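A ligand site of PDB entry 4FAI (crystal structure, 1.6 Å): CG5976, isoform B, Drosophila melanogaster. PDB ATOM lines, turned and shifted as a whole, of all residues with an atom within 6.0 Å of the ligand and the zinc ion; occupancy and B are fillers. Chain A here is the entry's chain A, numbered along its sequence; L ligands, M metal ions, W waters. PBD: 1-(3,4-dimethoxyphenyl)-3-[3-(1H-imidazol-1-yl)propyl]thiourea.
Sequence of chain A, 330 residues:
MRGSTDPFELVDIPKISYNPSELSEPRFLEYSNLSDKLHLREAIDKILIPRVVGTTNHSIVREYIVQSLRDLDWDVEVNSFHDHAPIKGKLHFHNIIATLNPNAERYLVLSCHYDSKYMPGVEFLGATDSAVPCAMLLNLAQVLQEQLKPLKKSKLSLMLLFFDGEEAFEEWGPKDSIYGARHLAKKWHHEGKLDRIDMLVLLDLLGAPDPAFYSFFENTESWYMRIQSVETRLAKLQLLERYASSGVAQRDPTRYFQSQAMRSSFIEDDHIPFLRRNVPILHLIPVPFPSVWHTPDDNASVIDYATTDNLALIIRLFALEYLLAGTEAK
NAV of the ligand lies close to OE2 of Glu 166 (3.2 Å).
The backbone carbonyl oxygen of Phe 266 lies close to a sulfur (SAC) of the ligand, at 3.8 Å.
CH2 of Trp 172 touches CAL of the ligand, at 3.5 Å.
OD2 of Asp 204 touches CAG of the ligand, at 3.3 Å.
Leu 205 touches the ligand (CD2 to CAD, 3.7 Å).
Ile 267 touches the ligand.
CD2 of Phe 289 touches OAP of the ligand, at 3.5 Å.
NE1 of Trp 293 touches NAM of the ligand (3.6 Å).
Along chain A the residues within 4 Å of the ligand span positions 129 to 294.
The backbone NH of Glu 268 sits close to a sulfur (SAC) of the ligand (3.3 Å).
Water W2 lies within hydrogen-bond range of an oxygen (OAQ) of the ligand and the backbone NH (N) of Phe 289.
The side-chain carboxylate (OD1) of Asp 129 lies within hydrogen-bond range of a ring nitrogen (NE2) of His 113, 2.8 Å away.
A ring nitrogen (NE2) of His 294 lies close to the indole nitrogen (NE1) of Trp 293, at 3.5 Å.
OE1 of Glu 268 is in hydrogen-bond range of NE1 of Trp 172 (2.8 Å).
The side-chain carboxylate (OD2) of Asp 204 lies close to the side-chain carboxylate (OD2) of Asp 269 (2.6 Å).
OG of Ser 130 lies within hydrogen-bond range of OD1 of Asp 204 (2.7 Å).
The zinc ion is bound by OD2 of Asp 129 (2.0 Å), NAM of the ligand (2.0 Å), OE1 of Glu 167 (2.0 Å) and NE2 of His 294 (2.1 Å).
Slightly farther from the zinc ion lies OD1 of Asp 129 (2.7 Å).
Trp 293 touches the zinc ion.
Four residues have an atom within 4 Å of the zinc ion: Asp 129, Glu 167, Trp 293 and His 294.
The nearest printed residue that does not touch the zinc ion is Glu 166 (4.2 Å).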
ATOM      1  N   HIS A 113      13.908   5.026   4.696  1.00  0.00           N
ATOM      2  CA  HIS A 113      12.874   4.863   5.701  1.00  0.00           C
ATOM      3  C   HIS A 113      11.472   4.941   5.111  1.00  0.00           C
ATOM      4  O   HIS A 113      11.254   5.695   4.185  1.00  0.00           O
ATOM      5  CB  HIS A 113      13.050   5.841   6.897  1.00  0.00           C
ATOM      6  CG  HIS A 113      12.631   7.257   6.648  1.00  0.00           C
ATOM      7  ND1 HIS A 113      11.380   7.714   6.978  1.00  0.00           N
ATOM      8  CD2 HIS A 113      13.319   8.324   6.160  1.00  0.00           C
ATOM      9  CE1 HIS A 113      11.291   8.995   6.646  1.00  0.00           C
ATOM     10  NE2 HIS A 113      12.463   9.393   6.199  1.00  0.00           N
ATOM     11  N   LYS A 117       6.893  11.475   9.115  1.00  0.00           N
ATOM     12  CA  LYS A 117       6.977  12.283  10.325  1.00  0.00           C
ATOM     13  C   LYS A 117       5.596  12.685  10.856  1.00  0.00           C
ATOM     14  O   LYS A 117       4.729  13.117  10.121  1.00  0.00           O
ATOM     15  CB  LYS A 117       7.794  13.526  10.071  1.00  0.00           C
ATOM     16  CG  LYS A 117       8.053  14.383  11.313  1.00  0.00           C
ATOM     17  CD  LYS A 117       9.170  15.395  11.064  1.00  0.00           C
ATOM     18  CE  LYS A 117       9.404  16.307  12.292  1.00  0.00           C
ATOM     19  NZ  LYS A 117       9.875  15.637  13.476  1.00  0.00           N
ATOM     20  N   PHE A 124       1.245  15.194   6.913  1.00  0.00           N
ATOM     21  CA  PHE A 124       2.554  15.338   6.299  1.00  0.00           C
ATOM     22  C   PHE A 124       2.808  14.108   5.448  1.00  0.00           C
ATOM     23  O   PHE A 124       2.857  13.000   5.957  1.00  0.00           O
ATOM     24  CB  PHE A 124       3.639  15.471   7.363  1.00  0.00           C
ATOM     25  CG  PHE A 124       5.018  15.491   6.797  1.00  0.00           C
ATOM     26  CD1 PHE A 124       5.458  16.571   6.056  1.00  0.00           C
ATOM     27  CD2 PHE A 124       5.872  14.404   6.990  1.00  0.00           C
ATOM     28  CE1 PHE A 124       6.759  16.604   5.550  1.00  0.00           C
ATOM     29  CE2 PHE A 124       7.169  14.419   6.472  1.00  0.00           C
ATOM     30  CZ  PHE A 124       7.601  15.504   5.741  1.00  0.00           C
ATOM     31  N   ASP A 129      10.812  12.434   1.510  1.00  0.00           N
ATOM     32  CA  ASP A 129      11.269  12.043   2.842  1.00  0.00           C
ATOM     33  C   ASP A 129      10.344  10.999   3.496  1.00  0.00           C
ATOM     34  O   ASP A 129       9.590  11.308   4.469  1.00  0.00           O
ATOM     35  CB  ASP A 129      11.327  13.345   3.687  1.00  0.00           C
ATOM     36  CG  ASP A 129      11.892  13.177   5.074  1.00  0.00           C
ATOM     37  OD1 ASP A 129      12.440  12.125   5.446  1.00  0.00           O
ATOM     38  OD2 ASP A 129      11.799  14.165   5.850  1.00  0.00           O
ATOM     39  N   SER A 130      10.323   9.754   3.022  1.00  0.00           N
ATOM     40  CA  SER A 130      11.101   9.193   1.924  1.00  0.00           C
ATOM     41  C   SER A 130      10.270   8.284   1.013  1.00  0.00           C
ATOM     42  O   SER A 130      10.691   7.198   0.581  1.00  0.00           O
ATOM     43  CB  SER A 130      12.319   8.431   2.497  1.00  0.00           C
ATOM     44  OG  SER A 130      13.287   9.371   2.914  1.00  0.00           O
ATOM     45  N   GLU A 166      12.349   6.208  11.525  1.00  0.00           N
ATOM     46  CA  GLU A 166      13.418   7.182  11.342  1.00  0.00           C
ATOM     47  C   GLU A 166      13.109   8.535  12.020  1.00  0.00           C
ATOM     48  O   GLU A 166      13.992   9.123  12.638  1.00  0.00           O
ATOM     49  CB  GLU A 166      13.733   7.385   9.866  1.00  0.00           C
ATOM     50  CG  GLU A 166      15.003   8.159   9.607  1.00  0.00           C
ATOM     51  CD  GLU A 166      14.802   9.662   9.401  1.00  0.00           C
ATOM     52  OE1 GLU A 166      13.654  10.166   9.534  1.00  0.00           O
ATOM     53  OE2 GLU A 166      15.807  10.334   9.110  1.00  0.00           O
ATOM     54  N   GLU A 167      11.870   9.013  11.895  1.00  0.00           N
ATOM     55  CA  GLU A 167      11.541  10.372  12.303  1.00  0.00           C
ATOM     56  C   GLU A 167      11.285  10.497  13.790  1.00  0.00           C
ATOM     57  O   GLU A 167      10.753   9.596  14.417  1.00  0.00           O
ATOM     58  CB  GLU A 167      10.319  10.878  11.542  1.00  0.00           C
ATOM     59  CG  GLU A 167      10.522  10.882  10.035  1.00  0.00           C
ATOM     60  CD  GLU A 167      11.293  12.042   9.524  1.00  0.00           C
ATOM     61  OE1 GLU A 167      11.299  12.218   8.298  1.00  0.00           O
ATOM     62  OE2 GLU A 167      11.934  12.787  10.327  1.00  0.00           O
ATOM     63  N   TRP A 172      14.001  16.021  17.412  1.00  0.00           N
ATOM     64  CA  TRP A 172      15.088  15.130  17.002  1.00  0.00           C
ATOM     65  C   TRP A 172      16.191  15.164  18.050  1.00  0.00           C
ATOM     66  O   TRP A 172      16.684  16.239  18.390  1.00  0.00           O
ATOM     67  CB  TRP A 172      15.665  15.534  15.638  1.00  0.00           C
ATOM     68  CG  TRP A 172      16.722  14.581  15.091  1.00  0.00           C
ATOM     69  CD1 TRP A 172      18.052  14.538  15.418  1.00  0.00           C
ATOM     70  CD2 TRP A 172      16.517  13.547  14.127  1.00  0.00           C
ATOM     71  NE1 TRP A 172      18.682  13.534  14.709  1.00  0.00           N
ATOM     72  CE2 TRP A 172      17.764  12.912  13.911  1.00  0.00           C
ATOM     73  CE3 TRP A 172      15.402  13.089  13.415  1.00  0.00           C
ATOM     74  CZ2 TRP A 172      17.918  11.858  13.006  1.00  0.00           C
ATOM     75  CZ3 TRP A 172      15.545  12.058  12.528  1.00  0.00           C
ATOM     76  CH2 TRP A 172      16.794  11.432  12.345  1.00  0.00           C
ATOM     77  N   ASP A 204      17.938   9.248   0.970  1.00  0.00           N
ATOM     78  CA  ASP A 204      17.034  10.084   1.779  1.00  0.00           C
ATOM     79  C   ASP A 204      16.865  11.427   1.058  1.00  0.00           C
ATOM     80  O   ASP A 204      17.808  11.910   0.439  1.00  0.00           O
ATOM     81  CB  ASP A 204      17.586  10.276   3.196  1.00  0.00           C
ATOM     82  CG  ASP A 204      16.497  10.612   4.214  1.00  0.00           C
ATOM     83  OD1 ASP A 204      15.357  10.927   3.811  1.00  0.00           O
ATOM     84  OD2 ASP A 204      16.772  10.537   5.429  1.00  0.00           O
ATOM     85  N   LEU A 205      15.670  11.997   1.140  1.00  0.00           N
ATOM     86  CA  LEU A 205      15.354  13.335   0.595  1.00  0.00           C
ATOM     87  C   LEU A 205      15.585  13.449  -0.924  1.00  0.00           C
ATOM     88  O   LEU A 205      16.177  14.413  -1.404  1.00  0.00           O
ATOM     89  CB  LEU A 205      16.147  14.389   1.398  1.00  0.00           C
ATOM     90  CG  LEU A 205      16.063  14.307   2.920  1.00  0.00           C
ATOM     91  CD1 LEU A 205      16.777  15.522   3.499  1.00  0.00           C
ATOM     92  CD2 LEU A 205      14.625  14.184   3.493  1.00  0.00           C
ATOM     93  N   PHE A 266      28.189  16.283   9.919  1.00  0.00           N
ATOM     94  CA  PHE A 266      27.669  15.387  10.951  1.00  0.00           C
ATOM     95  C   PHE A 266      26.162  15.266  10.797  1.00  0.00           C
ATOM     96  O   PHE A 266      25.416  15.490  11.768  1.00  0.00           O
ATOM     97  CB  PHE A 266      28.061  15.906  12.342  1.00  0.00           C
ATOM     98  CG  PHE A 266      29.548  15.898  12.586  1.00  0.00           C
ATOM     99  CD1 PHE A 266      30.281  17.084  12.537  1.00  0.00           C
ATOM    100  CD2 PHE A 266      30.215  14.705  12.829  1.00  0.00           C
ATOM    101  CE1 PHE A 266      31.662  17.073  12.757  1.00  0.00           C
ATOM    102  CE2 PHE A 266      31.599  14.686  13.045  1.00  0.00           C
ATOM    103  CZ  PHE A 266      32.318  15.872  13.014  1.00  0.00           C
ATOM    104  N   ILE A 267      25.721  14.921   9.577  1.00  0.00           N
ATOM    105  CA  ILE A 267      24.278  14.729   9.307  1.00  0.00           C
ATOM    106  C   ILE A 267      23.785  13.401   9.896  1.00  0.00           C
ATOM    107  O   ILE A 267      24.295  12.323   9.548  1.00  0.00           O
ATOM    108  CB  ILE A 267      23.911  14.720   7.814  1.00  0.00           C
ATOM    109  CG1 ILE A 267      24.370  16.023   7.131  1.00  0.00           C
ATOM    110  CG2 ILE A 267      22.389  14.519   7.658  1.00  0.00           C
ATOM    111  CD1 ILE A 267      24.190  16.021   5.615  1.00  0.00           C
ATOM    112  N   GLU A 268      22.803  13.476  10.775  1.00  0.00           N
ATOM    113  CA  GLU A 268      22.295  12.284  11.431  1.00  0.00           C
ATOM    114  C   GLU A 268      21.144  11.653  10.635  1.00  0.00           C
ATOM    115  O   GLU A 268      20.322  12.365  10.049  1.00  0.00           O
ATOM    116  CB  GLU A 268      21.818  12.631  12.816  1.00  0.00           C
ATOM    117  CG  GLU A 268      22.936  13.313  13.630  1.00  0.00           C
ATOM    118  CD  GLU A 268      22.576  13.475  15.077  1.00  0.00           C
ATOM    119  OE1 GLU A 268      21.358  13.482  15.394  1.00  0.00           O
ATOM    120  OE2 GLU A 268      23.517  13.590  15.890  1.00  0.00           O
ATOM    121  N   ASP A 269      21.114  10.328  10.571  1.00  0.00           N
ATOM    122  CA  ASP A 269      20.106   9.596   9.807  1.00  0.00           C
ATOM    123  C   ASP A 269      20.188   8.123  10.256  1.00  0.00           C
ATOM    124  O   ASP A 269      20.960   7.776  11.189  1.00  0.00           O
ATOM    125  CB  ASP A 269      20.381   9.738   8.295  1.00  0.00           C
ATOM    126  CG  ASP A 269      19.129   9.601   7.420  1.00  0.00           C
ATOM    127  OD1 ASP A 269      18.072   9.106   7.869  1.00  0.00           O
ATOM    128  OD2 ASP A 269      19.202  10.002   6.220  1.00  0.00           O
ATOM    129  N   ILE A 285      22.119  11.635   0.185  1.00  0.00           N
ATOM    130  CA  ILE A 285      21.260  12.706   0.685  1.00  0.00           C
ATOM    131  C   ILE A 285      21.823  14.043   0.137  1.00  0.00           C
ATOM    132  O   ILE A 285      23.027  14.298   0.229  1.00  0.00           O
ATOM    133  CB  ILE A 285      21.170  12.687   2.238  1.00  0.00           C
ATOM    134  CG1 ILE A 285      20.114  13.675   2.752  1.00  0.00           C
ATOM    135  CG2 ILE A 285      22.564  12.999   2.975  1.00  0.00           C
ATOM    136  CD1 ILE A 285      19.902  13.605   4.283  1.00  0.00           C
ATOM    137  N   PRO A 286      20.965  14.883  -0.456  1.00  0.00           N
ATOM    138  CA  PRO A 286      21.452  16.131  -1.042  1.00  0.00           C
ATOM    139  C   PRO A 286      21.776  17.145   0.065  1.00  0.00           C
ATOM    140  O   PRO A 286      21.204  17.086   1.151  1.00  0.00           O
ATOM    141  CB  PRO A 286      20.281  16.621  -1.897  1.00  0.00           C
ATOM    142  CG  PRO A 286      19.194  15.626  -1.725  1.00  0.00           C
ATOM    143  CD  PRO A 286      19.496  14.765  -0.541  1.00  0.00           C
ATOM    144  N   VAL A 287      22.742  18.017  -0.223  1.00  0.00           N
ATOM    145  CA  VAL A 287      23.067  19.139   0.645  1.00  0.00           C
ATOM    146  C   VAL A 287      23.228  20.377  -0.262  1.00  0.00           C
ATOM    147  O   VAL A 287      24.062  20.400  -1.166  1.00  0.00           O
ATOM    148  CB  VAL A 287      24.400  18.895   1.445  1.00  0.00           C
ATOM    149  CG1 VAL A 287      24.702  20.098   2.370  1.00  0.00           C
ATOM    150  CG2 VAL A 287      24.308  17.625   2.249  1.00  0.00           C
ATOM    151  N   PRO A 288      22.387  21.384  -0.057  1.00  0.00           N
ATOM    152  CA  PRO A 288      21.381  21.510   0.983  1.00  0.00           C
ATOM    153  C   PRO A 288      20.175  20.543   0.854  1.00  0.00           C
ATOM    154  O   PRO A 288      19.902  20.033  -0.216  1.00  0.00           O
ATOM    155  CB  PRO A 288      20.916  22.965   0.804  1.00  0.00           C
ATOM    156  CG  PRO A 288      21.013  23.185  -0.672  1.00  0.00           C
ATOM    157  CD  PRO A 288      22.297  22.484  -1.035  1.00  0.00           C
ATOM    158  N   PHE A 289      19.470  20.303   1.959  1.00  0.00           N
ATOM    159  CA  PHE A 289      18.207  19.555   1.912  1.00  0.00           C
ATOM    160  C   PHE A 289      17.214  20.339   1.053  1.00  0.00           C
ATOM    161  O   PHE A 289      17.304  21.561   0.967  1.00  0.00           O
ATOM    162  CB  PHE A 289      17.565  19.401   3.302  1.00  0.00           C
ATOM    163  CG  PHE A 289      18.313  18.514   4.279  1.00  0.00           C
ATOM    164  CD1 PHE A 289      19.491  17.865   3.950  1.00  0.00           C
ATOM    165  CD2 PHE A 289      17.779  18.314   5.544  1.00  0.00           C
ATOM    166  CE1 PHE A 289      20.131  17.082   4.880  1.00  0.00           C
ATOM    167  CE2 PHE A 289      18.397  17.529   6.470  1.00  0.00           C
ATOM    168  CZ  PHE A 289      19.581  16.883   6.134  1.00  0.00           C
ATOM    169  N   TRP A 293      11.690  20.737   3.172  1.00  0.00           N
ATOM    170  CA  TRP A 293      11.999  19.745   4.193  1.00  0.00           C
ATOM    171  C   TRP A 293      11.168  19.929   5.461  1.00  0.00           C
ATOM    172  O   TRP A 293      11.188  21.022   6.065  1.00  0.00           O
ATOM    173  CB  TRP A 293      13.493  19.786   4.537  1.00  0.00           C
ATOM    174  CG  TRP A 293      13.920  18.761   5.543  1.00  0.00           C
ATOM    175  CD1 TRP A 293      14.090  17.398   5.330  1.00  0.00           C
ATOM    176  CD2 TRP A 293      14.252  18.996   6.893  1.00  0.00           C
ATOM    177  NE1 TRP A 293      14.494  16.800   6.493  1.00  0.00           N
ATOM    178  CE2 TRP A 293      14.626  17.757   7.469  1.00  0.00           C
ATOM    179  CE3 TRP A 293      14.317  20.149   7.701  1.00  0.00           C
ATOM    180  CZ2 TRP A 293      15.007  17.640   8.791  1.00  0.00           C
ATOM    181  CZ3 TRP A 293      14.718  20.026   8.994  1.00  0.00           C
ATOM    182  CH2 TRP A 293      15.059  18.790   9.546  1.00  0.00           C
ATOM    183  N   HIS A 294      10.458  18.872   5.857  1.00  0.00           N
ATOM    184  CA  HIS A 294       9.626  18.877   7.077  1.00  0.00           C
ATOM    185  C   HIS A 294       8.545  19.973   7.090  1.00  0.00           C
ATOM    186  O   HIS A 294       8.175  20.480   8.140  1.00  0.00           O
ATOM    187  CB  HIS A 294      10.489  18.889   8.346  1.00  0.00           C
ATOM    188  CG  HIS A 294      11.190  17.578   8.601  1.00  0.00           C
ATOM    189  ND1 HIS A 294      11.896  17.303   9.757  1.00  0.00           N
ATOM    190  CD2 HIS A 294      11.250  16.453   7.845  1.00  0.00           C
ATOM    191  CE1 HIS A 294      12.387  16.074   9.689  1.00  0.00           C
ATOM    192  NE2 HIS A 294      12.007  15.538   8.542  1.00  0.00           N
HETATM  193  CAA PBD L   1      17.367  22.027   7.086  1.00  0.00           C
HETATM  194  CAB PBD L   1      22.573  20.190   6.068  1.00  0.00           C
HETATM  195  SAC PBD L   1      21.742  16.320  11.954  1.00  0.00           S
HETATM  196  CAD PBD L   1      15.251  13.049   6.930  1.00  0.00           C
HETATM  197  CAE PBD L   1      19.228  19.589   9.743  1.00  0.00           C
HETATM  198  CAF PBD L   1      18.591  20.344   8.772  1.00  0.00           C
HETATM  199  CAG PBD L   1      16.470  13.084   7.492  1.00  0.00           C
HETATM  200  CAH PBD L   1      15.029  13.742   8.993  1.00  0.00           C
HETATM  201  CAI PBD L   1      21.203  19.555   8.383  1.00  0.00           C
HETATM  202  CAJ PBD L   1      18.224  14.937   9.415  1.00  0.00           C
HETATM  203  CAK PBD L   1      19.402  15.222  10.374  1.00  0.00           C
HETATM  204  CAL PBD L   1      17.425  13.702   9.768  1.00  0.00           C
HETATM  205  NAM PBD L   1      14.346  13.460   7.865  1.00  0.00           N
HETATM  206  NAN PBD L   1      19.850  16.589  10.100  1.00  0.00           N
HETATM  207  NAO PBD L   1      21.187  18.449  10.462  1.00  0.00           N
HETATM  208  OAP PBD L   1      18.657  21.483   6.639  1.00  0.00           O
HETATM  209  OAQ PBD L   1      21.224  20.701   6.263  1.00  0.00           O
HETATM  210  CAR PBD L   1      20.853  17.188  10.756  1.00  0.00           C
HETATM  211  CAS PBD L   1      20.536  19.170   9.543  1.00  0.00           C
HETATM  212  CAT PBD L   1      19.259  20.721   7.608  1.00  0.00           C
HETATM  213  CAU PBD L   1      20.585  20.323   7.420  1.00  0.00           C
HETATM  214  NAV PBD L   1      16.318  13.516   8.767  1.00  0.00           N
HETATM  215 ZN    ZN M   1      12.401  13.727   7.653  1.00  0.00          ZN
HETATM  216  O   HOH W   1      23.028  21.018  11.807  1.00  0.00           O
HETATM  217  O   HOH W   2      20.086  21.953   4.138  1.00  0.00           O
